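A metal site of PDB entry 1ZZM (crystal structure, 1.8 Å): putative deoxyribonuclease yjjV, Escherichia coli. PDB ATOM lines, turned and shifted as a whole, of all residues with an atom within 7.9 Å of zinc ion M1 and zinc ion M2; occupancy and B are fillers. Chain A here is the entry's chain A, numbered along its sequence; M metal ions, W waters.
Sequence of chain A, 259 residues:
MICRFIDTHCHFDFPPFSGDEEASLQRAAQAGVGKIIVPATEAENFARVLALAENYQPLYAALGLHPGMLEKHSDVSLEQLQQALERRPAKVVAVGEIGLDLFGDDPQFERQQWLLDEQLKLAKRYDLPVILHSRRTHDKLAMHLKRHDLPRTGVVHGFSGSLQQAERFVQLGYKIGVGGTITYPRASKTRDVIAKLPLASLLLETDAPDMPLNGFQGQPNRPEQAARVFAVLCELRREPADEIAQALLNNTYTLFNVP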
ATOM      1  N   HIS A   9     -20.727  13.168  15.322  1.00  0.00           N
ATOM      2  CA  HIS A   9     -20.230  14.071  16.365  1.00  0.00           C
ATOM      3  C   HIS A   9     -20.290  13.361  17.728  1.00  0.00           C
ATOM      4  O   HIS A   9     -21.323  13.351  18.379  1.00  0.00           O
ATOM      5  CB  HIS A   9     -21.134  15.323  16.399  1.00  0.00           C
ATOM      6  CG  HIS A   9     -20.552  16.471  17.171  1.00  0.00           C
ATOM      7  ND1 HIS A   9     -19.994  17.569  16.558  1.00  0.00           N
ATOM      8  CD2 HIS A   9     -20.466  16.686  18.499  1.00  0.00           C
ATOM      9  CE1 HIS A   9     -19.587  18.422  17.497  1.00  0.00           C
ATOM     10  NE2 HIS A   9     -19.859  17.898  18.676  1.00  0.00           N
ATOM     11  N   CYS A  10     -19.196  12.737  18.119  1.00  0.00           N
ATOM     12  CA  CYS A  10     -19.154  12.075  19.404  1.00  0.00           C
ATOM     13  C   CYS A  10     -17.801  12.349  20.047  1.00  0.00           C
ATOM     14  O   CYS A  10     -16.751  12.098  19.445  1.00  0.00           O
ATOM     15  CB  CYS A  10     -19.347  10.553  19.227  1.00  0.00           C
ATOM     16  SG  CYS A  10     -19.212   9.634  20.832  1.00  0.00           S
ATOM     17  N   HIS A  11     -17.818  12.877  21.282  1.00  0.00           N
ATOM     18  CA  HIS A  11     -16.588  13.190  22.000  1.00  0.00           C
ATOM     19  C   HIS A  11     -16.119  11.896  22.655  1.00  0.00           C
ATOM     20  O   HIS A  11     -16.125  11.745  23.882  1.00  0.00           O
ATOM     21  CB  HIS A  11     -16.874  14.286  23.035  1.00  0.00           C
ATOM     22  CG  HIS A  11     -17.171  15.610  22.411  1.00  0.00           C
ATOM     23  ND1 HIS A  11     -16.189  16.422  21.901  1.00  0.00           N
ATOM     24  CD2 HIS A  11     -18.352  16.214  22.104  1.00  0.00           C
ATOM     25  CE1 HIS A  11     -16.732  17.459  21.294  1.00  0.00           C
ATOM     26  NE2 HIS A  11     -18.050  17.354  21.397  1.00  0.00           N
ATOM     27  N   PRO A  39     -14.615  15.018  17.191  1.00  0.00           N
ATOM     28  CA  PRO A  39     -14.038  16.360  17.069  1.00  0.00           C
ATOM     29  C   PRO A  39     -13.278  16.747  18.335  1.00  0.00           C
ATOM     30  O   PRO A  39     -13.773  16.514  19.455  1.00  0.00           O
ATOM     31  CB  PRO A  39     -15.248  17.229  16.808  1.00  0.00           C
ATOM     32  CG  PRO A  39     -16.358  16.545  17.531  1.00  0.00           C
ATOM     33  CD  PRO A  39     -16.044  15.067  17.552  1.00  0.00           C
ATOM     34  N   ALA A  40     -12.087  17.318  18.193  1.00  0.00           N
ATOM     35  CA  ALA A  40     -11.321  17.693  19.396  1.00  0.00           C
ATOM     36  C   ALA A  40     -11.895  18.963  19.999  1.00  0.00           C
ATOM     37  O   ALA A  40     -12.705  19.658  19.364  1.00  0.00           O
ATOM     38  CB  ALA A  40      -9.881  17.900  19.069  1.00  0.00           C
ATOM     39  N   THR A  41     -11.467  19.270  21.232  1.00  0.00           N
ATOM     40  CA  THR A  41     -11.921  20.461  21.960  1.00  0.00           C
ATOM     41  C   THR A  41     -10.811  21.444  22.263  1.00  0.00           C
ATOM     42  O   THR A  41     -11.059  22.638  22.495  1.00  0.00           O
ATOM     43  CB  THR A  41     -12.545  20.066  23.306  1.00  0.00           C
ATOM     44  OG1 THR A  41     -11.597  19.276  24.049  1.00  0.00           O
ATOM     45  CG2 THR A  41     -13.864  19.233  23.063  1.00  0.00           C
ATOM     46  N   HIS A  66     -12.505  24.346  20.635  1.00  0.00           N
ATOM     47  CA  HIS A  66     -13.895  24.549  21.057  1.00  0.00           C
ATOM     48  C   HIS A  66     -14.099  25.839  21.842  1.00  0.00           C
ATOM     49  O   HIS A  66     -13.303  26.177  22.726  1.00  0.00           O
ATOM     50  CB  HIS A  66     -14.301  23.306  21.887  1.00  0.00           C
ATOM     51  CG  HIS A  66     -15.783  23.125  22.052  1.00  0.00           C
ATOM     52  ND1 HIS A  66     -16.571  24.044  22.727  1.00  0.00           N
ATOM     53  CD2 HIS A  66     -16.595  22.082  21.754  1.00  0.00           C
ATOM     54  CE1 HIS A  66     -17.801  23.563  22.829  1.00  0.00           C
ATOM     55  NE2 HIS A  66     -17.838  22.373  22.257  1.00  0.00           N
ATOM     56  N   PRO A  67     -15.171  26.596  21.532  1.00  0.00           N
ATOM     57  CA  PRO A  67     -15.403  27.863  22.265  1.00  0.00           C
ATOM     58  C   PRO A  67     -15.608  27.652  23.762  1.00  0.00           C
ATOM     59  O   PRO A  67     -15.308  28.552  24.562  1.00  0.00           O
ATOM     60  CB  PRO A  67     -16.636  28.460  21.564  1.00  0.00           C
ATOM     61  CG  PRO A  67     -17.383  27.247  21.034  1.00  0.00           C
ATOM     62  CD  PRO A  67     -16.237  26.354  20.547  1.00  0.00           C
ATOM     63  N   GLU A  97     -14.299  21.004  15.974  1.00  0.00           N
ATOM     64  CA  GLU A  97     -15.200  21.528  16.930  1.00  0.00           C
ATOM     65  C   GLU A  97     -14.717  22.919  17.211  1.00  0.00           C
ATOM     66  O   GLU A  97     -13.883  23.162  18.070  1.00  0.00           O
ATOM     67  CB  GLU A  97     -15.681  20.782  18.159  1.00  0.00           C
ATOM     68  CG  GLU A  97     -17.062  21.500  18.325  1.00  0.00           C
ATOM     69  CD  GLU A  97     -18.103  20.854  19.221  1.00  0.00           C
ATOM     70  OE1 GLU A  97     -17.855  19.810  19.857  1.00  0.00           O
ATOM     71  OE2 GLU A  97     -19.212  21.428  19.260  1.00  0.00           O
ATOM     72  N   ILE A  98     -15.225  23.814  16.371  1.00  0.00           N
ATOM     73  CA  ILE A  98     -14.930  25.246  16.493  1.00  0.00           C
ATOM     74  C   ILE A  98     -16.319  25.877  16.463  1.00  0.00           C
ATOM     75  O   ILE A  98     -17.298  25.195  16.154  1.00  0.00           O
ATOM     76  CB  ILE A  98     -14.115  25.779  15.325  1.00  0.00           C
ATOM     77  CG1 ILE A  98     -14.930  25.705  14.026  1.00  0.00           C
ATOM     78  CG2 ILE A  98     -12.840  24.972  15.197  1.00  0.00           C
ATOM     79  CD1 ILE A  98     -14.119  26.072  12.792  1.00  0.00           C
ATOM     80  N   LEU A 100     -19.067  29.172  18.234  1.00  0.00           N
ATOM     81  CA  LEU A 100     -19.387  30.217  19.179  1.00  0.00           C
ATOM     82  C   LEU A 100     -20.401  29.730  20.194  1.00  0.00           C
ATOM     83  O   LEU A 100     -21.190  28.819  19.927  1.00  0.00           O
ATOM     84  CB  LEU A 100     -20.007  31.407  18.449  1.00  0.00           C
ATOM     85  CG  LEU A 100     -19.208  31.901  17.233  1.00  0.00           C
ATOM     86  CD1 LEU A 100     -20.124  32.752  16.430  1.00  0.00           C
ATOM     87  CD2 LEU A 100     -17.919  32.654  17.658  1.00  0.00           C
ATOM     88  N   ASP A 101     -20.415  30.347  21.368  1.00  0.00           N
ATOM     89  CA  ASP A 101     -21.344  29.896  22.403  1.00  0.00           C
ATOM     90  C   ASP A 101     -21.544  31.087  23.339  1.00  0.00           C
ATOM     91  O   ASP A 101     -20.596  31.502  24.013  1.00  0.00           O
ATOM     92  CB  ASP A 101     -20.691  28.730  23.127  1.00  0.00           C
ATOM     93  CG  ASP A 101     -21.593  28.076  24.159  1.00  0.00           C
ATOM     94  OD1 ASP A 101     -22.337  28.813  24.809  1.00  0.00           O
ATOM     95  OD2 ASP A 101     -21.556  26.830  24.305  1.00  0.00           O
ATOM     96  N   ILE A 131     -16.655  21.527  11.554  1.00  0.00           N
ATOM     97  CA  ILE A 131     -17.697  20.995  12.434  1.00  0.00           C
ATOM     98  C   ILE A 131     -17.899  22.140  13.405  1.00  0.00           C
ATOM     99  O   ILE A 131     -17.007  22.512  14.178  1.00  0.00           O
ATOM    100  CB  ILE A 131     -17.222  19.714  13.173  1.00  0.00           C
ATOM    101  CG1 ILE A 131     -17.249  18.534  12.180  1.00  0.00           C
ATOM    102  CG2 ILE A 131     -18.130  19.422  14.385  1.00  0.00           C
ATOM    103  CD1 ILE A 131     -16.765  17.166  12.810  1.00  0.00           C
ATOM    104  N   LEU A 132     -19.094  22.699  13.352  1.00  0.00           N
ATOM    105  CA  LEU A 132     -19.420  23.871  14.116  1.00  0.00           C
ATOM    106  C   LEU A 132     -20.379  23.693  15.275  1.00  0.00           C
ATOM    107  O   LEU A 132     -21.385  22.973  15.189  1.00  0.00           O
ATOM    108  CB  LEU A 132     -20.005  24.924  13.167  1.00  0.00           C
ATOM    109  CG  LEU A 132     -19.129  25.391  12.010  1.00  0.00           C
ATOM    110  CD1 LEU A 132     -20.033  25.981  10.897  1.00  0.00           C
ATOM    111  CD2 LEU A 132     -18.102  26.417  12.520  1.00  0.00           C
ATOM    112  N   HIS A 133     -20.046  24.419  16.350  1.00  0.00           N
ATOM    113  CA  HIS A 133     -20.815  24.494  17.582  1.00  0.00           C
ATOM    114  C   HIS A 133     -21.437  25.883  17.567  1.00  0.00           C
ATOM    115  O   HIS A 133     -20.763  26.879  17.246  1.00  0.00           O
ATOM    116  CB  HIS A 133     -19.876  24.393  18.790  1.00  0.00           C
ATOM    117  CG  HIS A 133     -20.560  24.512  20.121  1.00  0.00           C
ATOM    118  ND1 HIS A 133     -21.044  23.432  20.818  1.00  0.00           N
ATOM    119  CD2 HIS A 133     -20.777  25.585  20.921  1.00  0.00           C
ATOM    120  CE1 HIS A 133     -21.521  23.817  21.984  1.00  0.00           C
ATOM    121  NE2 HIS A 133     -21.382  25.126  22.071  1.00  0.00           N
ATOM    122  N   SER A 134     -22.724  25.974  17.903  1.00  0.00           N
ATOM    123  CA  SER A 134     -23.404  27.260  17.930  1.00  0.00           C
ATOM    124  C   SER A 134     -24.479  27.198  18.990  1.00  0.00           C
ATOM    125  O   SER A 134     -25.393  26.370  18.912  1.00  0.00           O
ATOM    126  CB  SER A 134     -24.036  27.583  16.577  1.00  0.00           C
ATOM    127  OG  SER A 134     -24.535  28.940  16.564  1.00  0.00           O
ATOM    128  N   ARG A 135     -24.372  28.050  19.992  1.00  0.00           N
ATOM    129  CA  ARG A 135     -25.374  28.027  21.028  1.00  0.00           C
ATOM    130  C   ARG A 135     -25.750  29.489  21.274  1.00  0.00           C
ATOM    131  O   ARG A 135     -24.959  30.265  21.857  1.00  0.00           O
ATOM    132  CB  ARG A 135     -24.779  27.394  22.275  1.00  0.00           C
ATOM    133  CG  ARG A 135     -25.692  27.449  23.474  1.00  0.00           C
ATOM    134  CD  ARG A 135     -24.842  27.284  24.713  1.00  0.00           C
ATOM    135  NE  ARG A 135     -25.363  26.264  25.591  1.00  0.00           N
ATOM    136  CZ  ARG A 135     -24.592  25.566  26.425  1.00  0.00           C
ATOM    137  NH1 ARG A 135     -23.280  25.805  26.446  1.00  0.00           N
ATOM    138  NH2 ARG A 135     -25.135  24.644  27.202  1.00  0.00           N
ATOM    139  N   HIS A 157     -23.474  21.521  13.970  1.00  0.00           N
ATOM    140  CA  HIS A 157     -23.902  20.354  14.757  1.00  0.00           C
ATOM    141  C   HIS A 157     -24.924  20.649  15.861  1.00  0.00           C
ATOM    142  O   HIS A 157     -25.099  21.795  16.282  1.00  0.00           O
ATOM    143  CB  HIS A 157     -22.654  19.685  15.345  1.00  0.00           C
ATOM    144  CG  HIS A 157     -22.503  19.876  16.826  1.00  0.00           C
ATOM    145  ND1 HIS A 157     -23.185  19.107  17.752  1.00  0.00           N
ATOM    146  CD2 HIS A 157     -21.805  20.797  17.537  1.00  0.00           C
ATOM    147  CE1 HIS A 157     -22.908  19.551  18.968  1.00  0.00           C
ATOM    148  NE2 HIS A 157     -22.073  20.569  18.870  1.00  0.00           N
ATOM    149  N   GLY A 158     -25.617  19.587  16.287  1.00  0.00           N
ATOM    150  CA  GLY A 158     -26.578  19.667  17.383  1.00  0.00           C
ATOM    151  C   GLY A 158     -27.502  20.852  17.282  1.00  0.00           C
ATOM    152  O   GLY A 158     -27.824  21.469  18.262  1.00  0.00           O
ATOM    153  N   GLU A 205     -26.202  12.531  14.537  1.00  0.00           N
ATOM    154  CA  GLU A 205     -25.147  12.645  15.565  1.00  0.00           C
ATOM    155  C   GLU A 205     -25.745  12.435  16.934  1.00  0.00           C
ATOM    156  O   GLU A 205     -26.969  12.294  17.055  1.00  0.00           O
ATOM    157  CB  GLU A 205     -24.543  14.046  15.581  1.00  0.00           C
ATOM    158  CG  GLU A 205     -25.545  15.081  16.112  1.00  0.00           C
ATOM    159  CD  GLU A 205     -24.965  16.471  16.248  1.00  0.00           C
ATOM    160  OE1 GLU A 205     -24.680  17.098  15.210  1.00  0.00           O
ATOM    161  OE2 GLU A 205     -24.823  16.953  17.379  1.00  0.00           O
ATOM    162  N   THR A 206     -24.880  12.418  17.950  1.00  0.00           N
ATOM    163  CA  THR A 206     -25.335  12.346  19.350  1.00  0.00           C
ATOM    164  C   THR A 206     -24.749  13.443  20.261  1.00  0.00           C
ATOM    165  O   THR A 206     -25.397  13.858  21.226  1.00  0.00           O
ATOM    166  CB  THR A 206     -24.952  11.032  20.089  1.00  0.00           C
ATOM    167  OG1 THR A 206     -23.523  10.887  20.091  1.00  0.00           O
ATOM    168  CG2 THR A 206     -25.645   9.793  19.450  1.00  0.00           C
ATOM    169  N   ASP A 207     -23.535  13.891  19.947  1.00  0.00           N
ATOM    170  CA  ASP A 207     -22.767  14.811  20.783  1.00  0.00           C
ATOM    171  C   ASP A 207     -22.492  14.089  22.116  1.00  0.00           C
ATOM    172  O   ASP A 207     -22.270  14.715  23.158  1.00  0.00           O
ATOM    173  CB  ASP A 207     -23.474  16.174  21.067  1.00  0.00           C
ATOM    174  CG  ASP A 207     -22.494  17.233  21.641  1.00  0.00           C
ATOM    175  OD1 ASP A 207     -21.267  17.067  21.493  1.00  0.00           O
ATOM    176  OD2 ASP A 207     -22.940  18.234  22.231  1.00  0.00           O
ATOM    177  N   ALA A 208     -22.509  12.756  22.109  1.00  0.00           N
ATOM    178  CA  ALA A 208     -22.238  12.019  23.358  1.00  0.00           C
ATOM    179  C   ALA A 208     -20.856  12.404  23.891  1.00  0.00           C
ATOM    180  O   ALA A 208     -19.908  12.579  23.128  1.00  0.00           O
ATOM    181  CB  ALA A 208     -22.304  10.491  23.118  1.00  0.00           C
ATOM    182  N   PRO A 209     -20.691  12.419  25.214  1.00  0.00           N
ATOM    183  CA  PRO A 209     -21.650  12.107  26.270  1.00  0.00           C
ATOM    184  C   PRO A 209     -22.671  13.167  26.618  1.00  0.00           C
ATOM    185  O   PRO A 209     -23.486  12.966  27.507  1.00  0.00           O
ATOM    186  CB  PRO A 209     -20.734  11.756  27.451  1.00  0.00           C
ATOM    187  CG  PRO A 209     -19.704  12.801  27.311  1.00  0.00           C
ATOM    188  CD  PRO A 209     -19.396  12.791  25.808  1.00  0.00           C
ATOM    189  N   ASP A 210     -22.642  14.321  25.948  1.00  0.00           N
ATOM    190  CA  ASP A 210     -23.639  15.347  26.291  1.00  0.00           C
ATOM    191  C   ASP A 210     -24.932  15.146  25.498  1.00  0.00           C
ATOM    192  O   ASP A 210     -25.049  14.170  24.742  1.00  0.00           O
ATOM    193  CB  ASP A 210     -23.065  16.750  26.021  1.00  0.00           C
ATOM    194  CG  ASP A 210     -21.799  17.031  26.844  1.00  0.00           C
ATOM    195  OD1 ASP A 210     -21.634  16.444  27.949  1.00  0.00           O
ATOM    196  OD2 ASP A 210     -20.967  17.856  26.396  1.00  0.00           O
ATOM    197  N   MET A 211     -25.905  16.054  25.682  1.00  0.00           N
ATOM    198  CA  MET A 211     -27.200  16.010  24.985  1.00  0.00           C
ATOM    199  C   MET A 211     -27.950  14.664  25.121  1.00  0.00           C
ATOM    200  O   MET A 211     -28.339  14.045  24.127  1.00  0.00           O
ATOM    201  CB  MET A 211     -26.998  16.407  23.503  1.00  0.00           C
ATOM    202  CG  MET A 211     -26.351  17.841  23.320  1.00  0.00           C
ATOM    203  SD  MET A 211     -26.100  18.535  21.583  1.00  0.00           S
ATOM    204  CE  MET A 211     -27.715  19.284  21.262  1.00  0.00           C
HETATM  205 ZN    ZN M   1     -19.328  18.639  20.554  1.00  0.00          ZN
HETATM  206 ZN    ZN M   2     -20.983  21.427  20.437  1.00  0.00          ZN
HETATM  207  O   HOH W   1     -22.836  21.101  21.963  1.00  0.00           O
HETATM  208  O   HOH W   2     -20.034  20.152  21.706  1.00  0.00           O
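N of His 133 lies within hydrogen-bond range of O of Ile 98 (2.9 Å).
The backbone NH of Leu 100 is in hydrogen-bond range of the backbone carbonyl oxygen of His 133.
OE2 of Glu 205 sits at hydrogen-bond distance from ND1 of His 157.
A ring nitrogen (NE2) of His 133 sits at hydrogen-bond distance from the side-chain carboxylate (OD2) of Asp 101 (2.8 Å).
The backbone carbonyl oxygen (O) of Ala 208 is in hydrogen-bond range of the backbone NH (N) of His 11 (2.8 Å).
NE2 of His 11 sits close to OD1 of Asp 207 (3.2 Å).
The backbone NH (N) of His 66 is in hydrogen-bond range of the backbone carbonyl oxygen (O) of Glu 97 (3.1 Å).
The backbone carbonyl oxygen of Leu 132 sits at hydrogen-bond distance from the backbone NH of His 157 (2.8 Å).
Within 4 Å of zinc ion M1: His 9, His 11, Glu 97, His 157 and Asp 207.
The nearest printed residue that does not touch zinc ion M1 is His 66 (4.4 Å).
His 66 touches zinc ion M2 (NE2 to ZN, 3.8 Å).
Zinc ion M1 is bound by NE2 of His 11, OE1 of Glu 97, water W2 and NE2 of His 9.
Slightly farther from zinc ion M1 lies OD1 of Asp 207 (2.7 Å).
Zinc ion M2 is bound by water W2 (2.0 Å), ND1 of His 133 (2.0 Å), NE2 of His 157 (2.1 Å), OE2 of Glu 97 (2.1 Å) and water W1 (2.4 Å).
Zinc ion M2 has five donor atoms within binding distance.
Water W2 bridges a ring nitrogen (NE2) of His 66 (3.2 Å) and the side-chain carboxylate (OD1) of Asp 207 (3.3 Å).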
